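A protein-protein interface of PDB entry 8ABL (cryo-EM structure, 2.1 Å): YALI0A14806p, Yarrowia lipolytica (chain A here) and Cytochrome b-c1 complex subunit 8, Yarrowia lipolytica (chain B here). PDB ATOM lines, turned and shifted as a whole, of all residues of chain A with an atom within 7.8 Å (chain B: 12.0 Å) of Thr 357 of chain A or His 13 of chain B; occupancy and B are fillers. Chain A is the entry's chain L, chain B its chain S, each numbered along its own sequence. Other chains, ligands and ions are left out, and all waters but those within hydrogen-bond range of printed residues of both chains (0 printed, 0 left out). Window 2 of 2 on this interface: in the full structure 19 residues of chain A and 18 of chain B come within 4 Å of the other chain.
The guanidinium group (NH1) of Arg 271 of chain A sits close to the side-chain amide nitrogen (NE2) of Gln 19 of chain B (3.5 Å).
The backbone NH (N) of Gly 12 of chain B is in hydrogen-bond range of the side-chain carboxylate (OE2) of Glu 457 of chain A.
The side-chain carboxylate (OE2) of Glu 457 of chain A sits at hydrogen-bond distance from the backbone NH (N) of His 13 of chain B, 2.9 Å away.
N of Met 14 of chain B is in hydrogen-bond range of OE2 of Glu 457 of chain A, at 2.6 Å.
OE2 of Glu 457 of chain A lies close to O of Trp 10 of chain B, 3.4 Å away.
The side-chain carboxylate of Glu 457 of chain A lies within salt-bridge range of the guanidinium group of Arg 271 of chain A (3.0 Å).
The side-chain amide oxygen (OD1) of Asn 355 of chain A is in hydrogen-bond range of the side-chain hydroxyl (OG1) of Thr 357 of chain A (3.5 Å).
The side-chain carboxylate (OD2) of Asp 360 of chain A is in hydrogen-bond range of the side-chain hydroxyl (OH) of Tyr 460 of chain A.
The backbone carbonyl oxygen of Met 14 of chain B sits at hydrogen-bond distance from the backbone NH of Gly 9 of chain B, at 2.9 Å.
The side-chain hydroxyl of Ser 16 of chain B lies within hydrogen-bond range of the side-chain amide nitrogen of Gln 19 of chain B (3.0 Å).
O of Thr 356 of chain A touches CA of Gly 12 of chain B (3.99 Å).
Thr 357 of chain A touches His 13 of chain B (CG2 to ND1, 3.8 Å).
Glu 457 of chain A touches Trp 11 of chain B (O to CE3, 3.7 Å).
Gly 458 of chain A touches Gly 12 of chain B (N to N, 3.9 Å).
Tyr 460 of chain A touches Trp 11 of chain B.
Leu 330 of chain A touches none of the printed residues of chain B.
No residue of chain B comes within 4 Å of Asn 355 of chain A.
Of the printed residues of chain B, Thr 356 of chain A touches Gly 12.
Of the printed residues of chain B, Thr 357 of chain A touches His 13.
No residue of chain B comes within 4 Å of Ile 359 of chain A.
No residue of chain B comes within 4 Å of Asp 360 of chain A.
Gly 458 of chain A touches just one residue of chain B: Gly 12.
Gly 9 of chain B touches none of the printed residues of chain A.
Of chain A, only Thr 357 and Glu 457 come within 4 Å of His 13 of chain B.
Of the printed residues of chain A, Met 14 of chain B touches Glu 457 (2.6 Å).
The nearest residue of chain B that does not touch Thr 357 of chain A is Trp 11 of chain B (4.3 Å).
Printed residues of chain B that touch a printed residue of chain A: Trp 10, Trp 11, Gly 12, His 13, Met 14 and Gln 19.
Hydrophobic or aromatic side chains of chain B within 4 Å of the printed part of chain A: Trp 11, His 13 and Met 14.
Among the printed residues, no Asp or Glu carboxylate lies within 4 Å of a Lys or Arg side-chain nitrogen of the other chain.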
ATOM      1  N   ARG A 271     -15.796 -27.645 -21.363  1.00  0.00           N
ATOM      2  CA  ARG A 271     -17.206 -27.505 -21.651  1.00  0.00           C
ATOM      3  C   ARG A 271     -17.935 -26.962 -20.425  1.00  0.00           C
ATOM      4  O   ARG A 271     -17.686 -27.412 -19.315  1.00  0.00           O
ATOM      5  CB  ARG A 271     -17.785 -28.857 -22.045  1.00  0.00           C
ATOM      6  CG  ARG A 271     -19.289 -28.826 -22.234  1.00  0.00           C
ATOM      7  CD  ARG A 271     -19.644 -30.027 -23.080  1.00  0.00           C
ATOM      8  NE  ARG A 271     -21.083 -30.190 -23.037  1.00  0.00           N
ATOM      9  CZ  ARG A 271     -21.759 -31.177 -23.609  1.00  0.00           C
ATOM     10  NH1 ARG A 271     -21.126 -32.122 -24.287  1.00  0.00           N
ATOM     11  NH2 ARG A 271     -23.073 -31.210 -23.476  1.00  0.00           N
ATOM     12  N   LEU A 330     -23.318 -16.548 -37.634  1.00  0.00           N
ATOM     13  CA  LEU A 330     -22.646 -17.688 -37.060  1.00  0.00           C
ATOM     14  C   LEU A 330     -21.906 -17.299 -35.791  1.00  0.00           C
ATOM     15  O   LEU A 330     -21.542 -18.186 -35.047  1.00  0.00           O
ATOM     16  CB  LEU A 330     -21.718 -18.340 -38.084  1.00  0.00           C
ATOM     17  CG  LEU A 330     -22.404 -18.935 -39.311  1.00  0.00           C
ATOM     18  CD1 LEU A 330     -21.367 -19.456 -40.297  1.00  0.00           C
ATOM     19  CD2 LEU A 330     -23.402 -20.032 -38.933  1.00  0.00           C
ATOM     20  N   SER A 353     -19.388 -17.136 -29.960  1.00  0.00           N
ATOM     21  CA  SER A 353     -20.637 -17.430 -30.649  1.00  0.00           C
ATOM     22  C   SER A 353     -21.705 -17.860 -29.653  1.00  0.00           C
ATOM     23  O   SER A 353     -21.415 -18.574 -28.704  1.00  0.00           O
ATOM     24  CB  SER A 353     -20.420 -18.499 -31.691  1.00  0.00           C
ATOM     25  OG  SER A 353     -21.648 -18.889 -32.284  1.00  0.00           O
ATOM     26  N   GLU A 354     -22.952 -17.442 -29.890  1.00  0.00           N
ATOM     27  CA  GLU A 354     -24.087 -17.937 -29.126  1.00  0.00           C
ATOM     28  C   GLU A 354     -24.828 -18.991 -29.941  1.00  0.00           C
ATOM     29  O   GLU A 354     -25.812 -19.557 -29.475  1.00  0.00           O
ATOM     30  CB  GLU A 354     -25.078 -16.811 -28.850  1.00  0.00           C
ATOM     31  CG  GLU A 354     -24.665 -15.895 -27.719  1.00  0.00           C
ATOM     32  CD  GLU A 354     -25.090 -14.430 -27.780  1.00  0.00           C
ATOM     33  OE1 GLU A 354     -24.688 -13.674 -26.857  1.00  0.00           O
ATOM     34  OE2 GLU A 354     -25.807 -14.041 -28.742  1.00  0.00           O
ATOM     35  N   ASN A 355     -24.409 -19.197 -31.186  1.00  0.00           N
ATOM     36  CA  ASN A 355     -25.132 -20.099 -32.064  1.00  0.00           C
ATOM     37  C   ASN A 355     -24.586 -21.498 -31.819  1.00  0.00           C
ATOM     38  O   ASN A 355     -23.637 -21.932 -32.475  1.00  0.00           O
ATOM     39  CB  ASN A 355     -25.010 -19.661 -33.524  1.00  0.00           C
ATOM     40  CG  ASN A 355     -25.987 -20.310 -34.486  1.00  0.00           C
ATOM     41  OD1 ASN A 355     -26.607 -21.335 -34.191  1.00  0.00           O
ATOM     42  ND2 ASN A 355     -26.137 -19.698 -35.656  1.00  0.00           N
ATOM     43  N   THR A 356     -25.155 -22.176 -30.825  1.00  0.00           N
ATOM     44  CA  THR A 356     -24.523 -23.387 -30.329  1.00  0.00           C
ATOM     45  C   THR A 356     -24.763 -24.574 -31.259  1.00  0.00           C
ATOM     46  O   THR A 356     -24.019 -25.550 -31.201  1.00  0.00           O
ATOM     47  CB  THR A 356     -24.997 -23.716 -28.911  1.00  0.00           C
ATOM     48  OG1 THR A 356     -26.407 -23.930 -28.981  1.00  0.00           O
ATOM     49  CG2 THR A 356     -24.686 -22.603 -27.936  1.00  0.00           C
ATOM     50  N   THR A 357     -25.793 -24.499 -32.106  1.00  0.00           N
ATOM     51  CA  THR A 357     -26.074 -25.588 -33.027  1.00  0.00           C
ATOM     52  C   THR A 357     -25.326 -25.410 -34.343  1.00  0.00           C
ATOM     53  O   THR A 357     -25.280 -26.358 -35.122  1.00  0.00           O
ATOM     54  CB  THR A 357     -27.574 -25.740 -33.292  1.00  0.00           C
ATOM     55  OG1 THR A 357     -27.977 -24.492 -33.859  1.00  0.00           O
ATOM     56  CG2 THR A 357     -28.348 -26.050 -32.027  1.00  0.00           C
ATOM     57  N   GLN A 358     -24.704 -24.245 -34.557  1.00  0.00           N
ATOM     58  CA  GLN A 358     -23.979 -24.059 -35.803  1.00  0.00           C
ATOM     59  C   GLN A 358     -22.508 -23.765 -35.556  1.00  0.00           C
ATOM     60  O   GLN A 358     -21.853 -23.124 -36.376  1.00  0.00           O
ATOM     61  CB  GLN A 358     -24.616 -22.973 -36.664  1.00  0.00           C
ATOM     62  CG  GLN A 358     -25.954 -23.403 -37.236  1.00  0.00           C
ATOM     63  CD  GLN A 358     -26.399 -22.391 -38.254  1.00  0.00           C
ATOM     64  OE1 GLN A 358     -27.127 -21.455 -37.935  1.00  0.00           O
ATOM     65  NE2 GLN A 358     -25.883 -22.527 -39.467  1.00  0.00           N
ATOM     66  N   ILE A 359     -21.994 -24.245 -34.429  1.00  0.00           N
ATOM     67  CA  ILE A 359     -20.584 -24.078 -34.149  1.00  0.00           C
ATOM     68  C   ILE A 359     -19.780 -24.806 -35.230  1.00  0.00           C
ATOM     69  O   ILE A 359     -18.764 -24.295 -35.712  1.00  0.00           O
ATOM     70  CB  ILE A 359     -20.267 -24.588 -32.737  1.00  0.00           C
ATOM     71  CG1 ILE A 359     -20.738 -23.582 -31.682  1.00  0.00           C
ATOM     72  CG2 ILE A 359     -18.781 -24.915 -32.625  1.00  0.00           C
ATOM     73  CD1 ILE A 359     -20.541 -24.063 -30.267  1.00  0.00           C
ATOM     74  N   ASP A 360     -20.265 -25.990 -35.626  1.00  0.00           N
ATOM     75  CA  ASP A 360     -19.656 -26.757 -36.700  1.00  0.00           C
ATOM     76  C   ASP A 360     -19.527 -25.923 -37.980  1.00  0.00           C
ATOM     77  O   ASP A 360     -18.453 -25.890 -38.575  1.00  0.00           O
ATOM     78  CB  ASP A 360     -20.348 -28.105 -36.901  1.00  0.00           C
ATOM     79  CG  ASP A 360     -21.734 -28.011 -37.511  1.00  0.00           C
ATOM     80  OD1 ASP A 360     -22.549 -27.241 -36.979  1.00  0.00           O
ATOM     81  OD2 ASP A 360     -21.981 -28.731 -38.506  1.00  0.00           O
ATOM     82  N   ASP A 361     -20.584 -25.197 -38.368  1.00  0.00           N
ATOM     83  CA  ASP A 361     -20.544 -24.338 -39.545  1.00  0.00           C
ATOM     84  C   ASP A 361     -19.511 -23.229 -39.370  1.00  0.00           C
ATOM     85  O   ASP A 361     -18.698 -22.991 -40.261  1.00  0.00           O
ATOM     86  CB  ASP A 361     -21.919 -23.770 -39.892  1.00  0.00           C
ATOM     87  CG  ASP A 361     -22.894 -24.839 -40.354  1.00  0.00           C
ATOM     88  OD1 ASP A 361     -22.460 -25.792 -41.048  1.00  0.00           O
ATOM     89  OD2 ASP A 361     -24.078 -24.743 -39.987  1.00  0.00           O
ATOM     90  N   LEU A 362     -19.525 -22.574 -38.211  1.00  0.00           N
ATOM     91  CA  LEU A 362     -18.591 -21.490 -37.989  1.00  0.00           C
ATOM     92  C   LEU A 362     -17.152 -21.980 -38.193  1.00  0.00           C
ATOM     93  O   LEU A 362     -16.392 -21.360 -38.935  1.00  0.00           O
ATOM     94  CB  LEU A 362     -18.831 -20.933 -36.585  1.00  0.00           C
ATOM     95  CG  LEU A 362     -17.800 -19.920 -36.094  1.00  0.00           C
ATOM     96  CD1 LEU A 362     -17.785 -18.668 -36.972  1.00  0.00           C
ATOM     97  CD2 LEU A 362     -18.086 -19.554 -34.647  1.00  0.00           C
ATOM     98  N   PRO A 455     -20.513 -23.680 -24.068  1.00  0.00           N
ATOM     99  CA  PRO A 455     -21.408 -24.698 -24.625  1.00  0.00           C
ATOM    100  C   PRO A 455     -20.884 -25.223 -25.963  1.00  0.00           C
ATOM    101  O   PRO A 455     -21.353 -24.823 -27.022  1.00  0.00           O
ATOM    102  CB  PRO A 455     -22.719 -23.903 -24.745  1.00  0.00           C
ATOM    103  CG  PRO A 455     -22.254 -22.497 -25.069  1.00  0.00           C
ATOM    104  CD  PRO A 455     -21.029 -22.308 -24.202  1.00  0.00           C
ATOM    105  N   GLU A 457     -20.671 -28.478 -27.052  1.00  0.00           N
ATOM    106  CA  GLU A 457     -21.094 -29.802 -27.485  1.00  0.00           C
ATOM    107  C   GLU A 457     -21.035 -29.919 -29.012  1.00  0.00           C
ATOM    108  O   GLU A 457     -20.613 -30.948 -29.525  1.00  0.00           O
ATOM    109  CB  GLU A 457     -22.497 -30.128 -26.981  1.00  0.00           C
ATOM    110  CG  GLU A 457     -22.978 -31.505 -27.413  1.00  0.00           C
ATOM    111  CD  GLU A 457     -24.406 -31.813 -27.005  1.00  0.00           C
ATOM    112  OE1 GLU A 457     -24.628 -32.196 -25.832  1.00  0.00           O
ATOM    113  OE2 GLU A 457     -25.297 -31.647 -27.859  1.00  0.00           O
ATOM    114  N   GLY A 458     -21.428 -28.857 -29.731  1.00  0.00           N
ATOM    115  CA  GLY A 458     -21.386 -28.820 -31.187  1.00  0.00           C
ATOM    116  C   GLY A 458     -19.979 -28.716 -31.780  1.00  0.00           C
ATOM    117  O   GLY A 458     -19.818 -28.711 -32.997  1.00  0.00           O
ATOM    118  N   TYR A 460     -16.889 -30.370 -33.087  1.00  0.00           N
ATOM    119  CA  TYR A 460     -16.552 -31.767 -33.349  1.00  0.00           C
ATOM    120  C   TYR A 460     -15.194 -32.129 -32.756  1.00  0.00           C
ATOM    121  O   TYR A 460     -14.446 -31.252 -32.336  1.00  0.00           O
ATOM    122  CB  TYR A 460     -16.545 -32.063 -34.846  1.00  0.00           C
ATOM    123  CG  TYR A 460     -17.909 -32.010 -35.488  1.00  0.00           C
ATOM    124  CD1 TYR A 460     -19.017 -32.556 -34.853  1.00  0.00           C
ATOM    125  CD2 TYR A 460     -18.098 -31.422 -36.731  1.00  0.00           C
ATOM    126  CE1 TYR A 460     -20.278 -32.512 -35.429  1.00  0.00           C
ATOM    127  CE2 TYR A 460     -19.354 -31.376 -37.328  1.00  0.00           C
ATOM    128  CZ  TYR A 460     -20.452 -31.909 -36.666  1.00  0.00           C
ATOM    129  OH  TYR A 460     -21.707 -31.898 -37.209  1.00  0.00           O
ATOM    130  N   TYR B   7     -35.036 -39.616 -27.015  1.00  0.00           N
ATOM    131  CA  TYR B   7     -33.899 -39.855 -26.035  1.00  0.00           C
ATOM    132  C   TYR B   7     -32.530 -39.538 -26.630  1.00  0.00           C
ATOM    133  O   TYR B   7     -31.502 -39.714 -25.974  1.00  0.00           O
ATOM    134  CB  TYR B   7     -33.956 -41.268 -25.452  1.00  0.00           C
ATOM    135  CG  TYR B   7     -35.181 -41.481 -24.606  1.00  0.00           C
ATOM    136  CD1 TYR B   7     -35.304 -40.867 -23.366  1.00  0.00           C
ATOM    137  CD2 TYR B   7     -36.249 -42.240 -25.069  1.00  0.00           C
ATOM    138  CE1 TYR B   7     -36.448 -41.020 -22.596  1.00  0.00           C
ATOM    139  CE2 TYR B   7     -37.396 -42.407 -24.308  1.00  0.00           C
ATOM    140  CZ  TYR B   7     -37.495 -41.797 -23.067  1.00  0.00           C
ATOM    141  OH  TYR B   7     -38.622 -41.957 -22.317  1.00  0.00           O
ATOM    142  N   MET B   8     -32.494 -39.083 -27.876  1.00  0.00           N
ATOM    143  CA  MET B   8     -31.246 -38.528 -28.364  1.00  0.00           C
ATOM    144  C   MET B   8     -31.592 -37.266 -29.138  1.00  0.00           C
ATOM    145  O   MET B   8     -32.555 -37.279 -29.892  1.00  0.00           O
ATOM    146  CB  MET B   8     -30.511 -39.526 -29.264  1.00  0.00           C
ATOM    147  CG  MET B   8     -29.164 -38.998 -29.746  1.00  0.00           C
ATOM    148  SD  MET B   8     -28.273 -40.129 -30.852  1.00  0.00           S
ATOM    149  CE  MET B   8     -29.189 -39.919 -32.380  1.00  0.00           C
ATOM    150  N   GLY B   9     -30.836 -36.181 -28.942  1.00  0.00           N
ATOM    151  CA  GLY B   9     -31.070 -35.012 -29.771  1.00  0.00           C
ATOM    152  C   GLY B   9     -30.085 -35.005 -30.933  1.00  0.00           C
ATOM    153  O   GLY B   9     -30.003 -35.972 -31.684  1.00  0.00           O
ATOM    154  N   TRP B  10     -29.335 -33.911 -31.058  1.00  0.00           N
ATOM    155  CA  TRP B  10     -28.361 -33.769 -32.127  1.00  0.00           C
ATOM    156  C   TRP B  10     -27.228 -32.887 -31.617  1.00  0.00           C
ATOM    157  O   TRP B  10     -27.308 -32.382 -30.504  1.00  0.00           O
ATOM    158  CB  TRP B  10     -29.027 -33.183 -33.376  1.00  0.00           C
ATOM    159  CG  TRP B  10     -28.292 -33.539 -34.634  1.00  0.00           C
ATOM    160  CD1 TRP B  10     -27.533 -32.718 -35.419  1.00  0.00           C
ATOM    161  CD2 TRP B  10     -28.218 -34.848 -35.235  1.00  0.00           C
ATOM    162  NE1 TRP B  10     -26.998 -33.422 -36.471  1.00  0.00           N
ATOM    163  CE2 TRP B  10     -27.410 -34.729 -36.393  1.00  0.00           C
ATOM    164  CE3 TRP B  10     -28.764 -36.102 -34.910  1.00  0.00           C
ATOM    165  CZ2 TRP B  10     -27.148 -35.819 -37.230  1.00  0.00           C
ATOM    166  CZ3 TRP B  10     -28.519 -37.175 -35.748  1.00  0.00           C
ATOM    167  CH2 TRP B  10     -27.719 -37.033 -36.891  1.00  0.00           C
ATOM    168  N   TRP B  11     -26.178 -32.681 -32.412  1.00  0.00           N
ATOM    169  CA  TRP B  11     -25.067 -31.868 -31.940  1.00  0.00           C
ATOM    170  C   TRP B  11     -25.538 -30.508 -31.417  1.00  0.00           C
ATOM    171  O   TRP B  11     -26.280 -29.801 -32.092  1.00  0.00           O
ATOM    172  CB  TRP B  11     -24.069 -31.704 -33.071  1.00  0.00           C
ATOM    173  CG  TRP B  11     -23.543 -33.023 -33.537  1.00  0.00           C
ATOM    174  CD1 TRP B  11     -23.884 -33.683 -34.685  1.00  0.00           C
ATOM    175  CD2 TRP B  11     -22.582 -33.852 -32.851  1.00  0.00           C
ATOM    176  NE1 TRP B  11     -23.180 -34.857 -34.773  1.00  0.00           N
ATOM    177  CE2 TRP B  11     -22.372 -34.989 -33.666  1.00  0.00           C
ATOM    178  CE3 TRP B  11     -21.868 -33.744 -31.642  1.00  0.00           C
ATOM    179  CZ2 TRP B  11     -21.476 -36.006 -33.301  1.00  0.00           C
ATOM    180  CZ3 TRP B  11     -20.979 -34.745 -31.284  1.00  0.00           C
ATOM    181  CH2 TRP B  11     -20.792 -35.863 -32.108  1.00  0.00           C
ATOM    182  N   GLY B  12     -25.109 -30.145 -30.202  1.00  0.00           N
ATOM    183  CA  GLY B  12     -25.527 -28.884 -29.615  1.00  0.00           C
ATOM    184  C   GLY B  12     -26.696 -29.048 -28.645  1.00  0.00           C
ATOM    185  O   GLY B  12     -26.845 -28.237 -27.738  1.00  0.00           O
ATOM    186  N   HIS B  13     -27.504 -30.097 -28.811  1.00  0.00           N
ATOM    187  CA  HIS B  13     -28.594 -30.371 -27.889  1.00  0.00           C
ATOM    188  C   HIS B  13     -28.765 -31.879 -27.802  1.00  0.00           C
ATOM    189  O   HIS B  13     -29.822 -32.408 -28.132  1.00  0.00           O
ATOM    190  CB  HIS B  13     -29.881 -29.649 -28.335  1.00  0.00           C
ATOM    191  CG  HIS B  13     -30.276 -29.943 -29.746  1.00  0.00           C
ATOM    192  ND1 HIS B  13     -29.643 -29.358 -30.821  1.00  0.00           N
ATOM    193  CD2 HIS B  13     -31.216 -30.769 -30.265  1.00  0.00           C
ATOM    194  CE1 HIS B  13     -30.181 -29.799 -31.942  1.00  0.00           C
ATOM    195  NE2 HIS B  13     -31.140 -30.685 -31.627  1.00  0.00           N
ATOM    196  N   MET B  14     -27.703 -32.574 -27.392  1.00  0.00           N
ATOM    197  CA  MET B  14     -27.710 -34.027 -27.476  1.00  0.00           C
ATOM    198  C   MET B  14     -28.665 -34.641 -26.446  1.00  0.00           C
ATOM    199  O   MET B  14     -29.148 -35.749 -26.659  1.00  0.00           O
ATOM    200  CB  MET B  14     -26.307 -34.622 -27.324  1.00  0.00           C
ATOM    201  CG  MET B  14     -26.180 -36.042 -27.867  1.00  0.00           C
ATOM    202  SD  MET B  14     -26.344 -36.114 -29.673  1.00  0.00           S
ATOM    203  CE  MET B  14     -24.847 -35.255 -30.163  1.00  0.00           C
ATOM    204  N   GLY B  15     -28.977 -33.910 -25.367  1.00  0.00           N
ATOM    205  CA  GLY B  15     -29.826 -34.426 -24.298  1.00  0.00           C
ATOM    206  C   GLY B  15     -29.043 -34.832 -23.048  1.00  0.00           C
ATOM    207  O   GLY B  15     -29.602 -35.424 -22.126  1.00  0.00           O
ATOM    208  N   SER B  16     -27.756 -34.473 -23.006  1.00  0.00           N
ATOM    209  CA  SER B  16     -26.914 -34.630 -21.832  1.00  0.00           C
ATOM    210  C   SER B  16     -27.458 -33.775 -20.692  1.00  0.00           C
ATOM    211  O   SER B  16     -27.921 -32.665 -20.924  1.00  0.00           O
ATOM    212  CB  SER B  16     -25.520 -34.208 -22.188  1.00  0.00           C
ATOM    213  OG  SER B  16     -24.683 -34.146 -21.045  1.00  0.00           O
ATOM    214  N   PRO B  17     -27.370 -34.215 -19.419  1.00  0.00           N
ATOM    215  CA  PRO B  17     -27.499 -33.277 -18.305  1.00  0.00           C
ATOM    216  C   PRO B  17     -26.406 -32.232 -18.504  1.00  0.00           C
ATOM    217  O   PRO B  17     -25.393 -32.503 -19.148  1.00  0.00           O
ATOM    218  CB  PRO B  17     -27.135 -34.114 -17.075  1.00  0.00           C
ATOM    219  CG  PRO B  17     -27.415 -35.528 -17.512  1.00  0.00           C
ATOM    220  CD  PRO B  17     -27.059 -35.582 -18.982  1.00  0.00           C
ATOM    221  N   PRO B  18     -26.577 -31.001 -17.980  1.00  0.00           N
ATOM    222  CA  PRO B  18     -25.561 -29.960 -18.121  1.00  0.00           C
ATOM    223  C   PRO B  18     -24.192 -30.456 -17.676  1.00  0.00           C
ATOM    224  O   PRO B  18     -24.066 -31.125 -16.657  1.00  0.00           O
ATOM    225  CB  PRO B  18     -26.014 -28.894 -17.124  1.00  0.00           C
ATOM    226  CG  PRO B  18     -27.506 -29.078 -17.044  1.00  0.00           C
ATOM    227  CD  PRO B  18     -27.756 -30.558 -17.217  1.00  0.00           C
ATOM    228  N   GLN B  19     -23.180 -30.150 -18.478  1.00  0.00           N
ATOM    229  CA  GLN B  19     -21.833 -30.550 -18.123  1.00  0.00           C
ATOM    230  C   GLN B  19     -21.072 -29.318 -17.653  1.00  0.00           C
ATOM    231  O   GLN B  19     -21.194 -28.240 -18.232  1.00  0.00           O
ATOM    232  CB  GLN B  19     -21.135 -31.204 -19.312  1.00  0.00           C
ATOM    233  CG  GLN B  19     -21.924 -32.363 -19.915  1.00  0.00           C
ATOM    234  CD  GLN B  19     -21.098 -33.207 -20.862  1.00  0.00           C
ATOM    235  OE1 GLN B  19     -19.887 -33.029 -20.992  1.00  0.00           O
ATOM    236  NE2 GLN B  19     -21.746 -34.149 -21.529  1.00  0.00           N
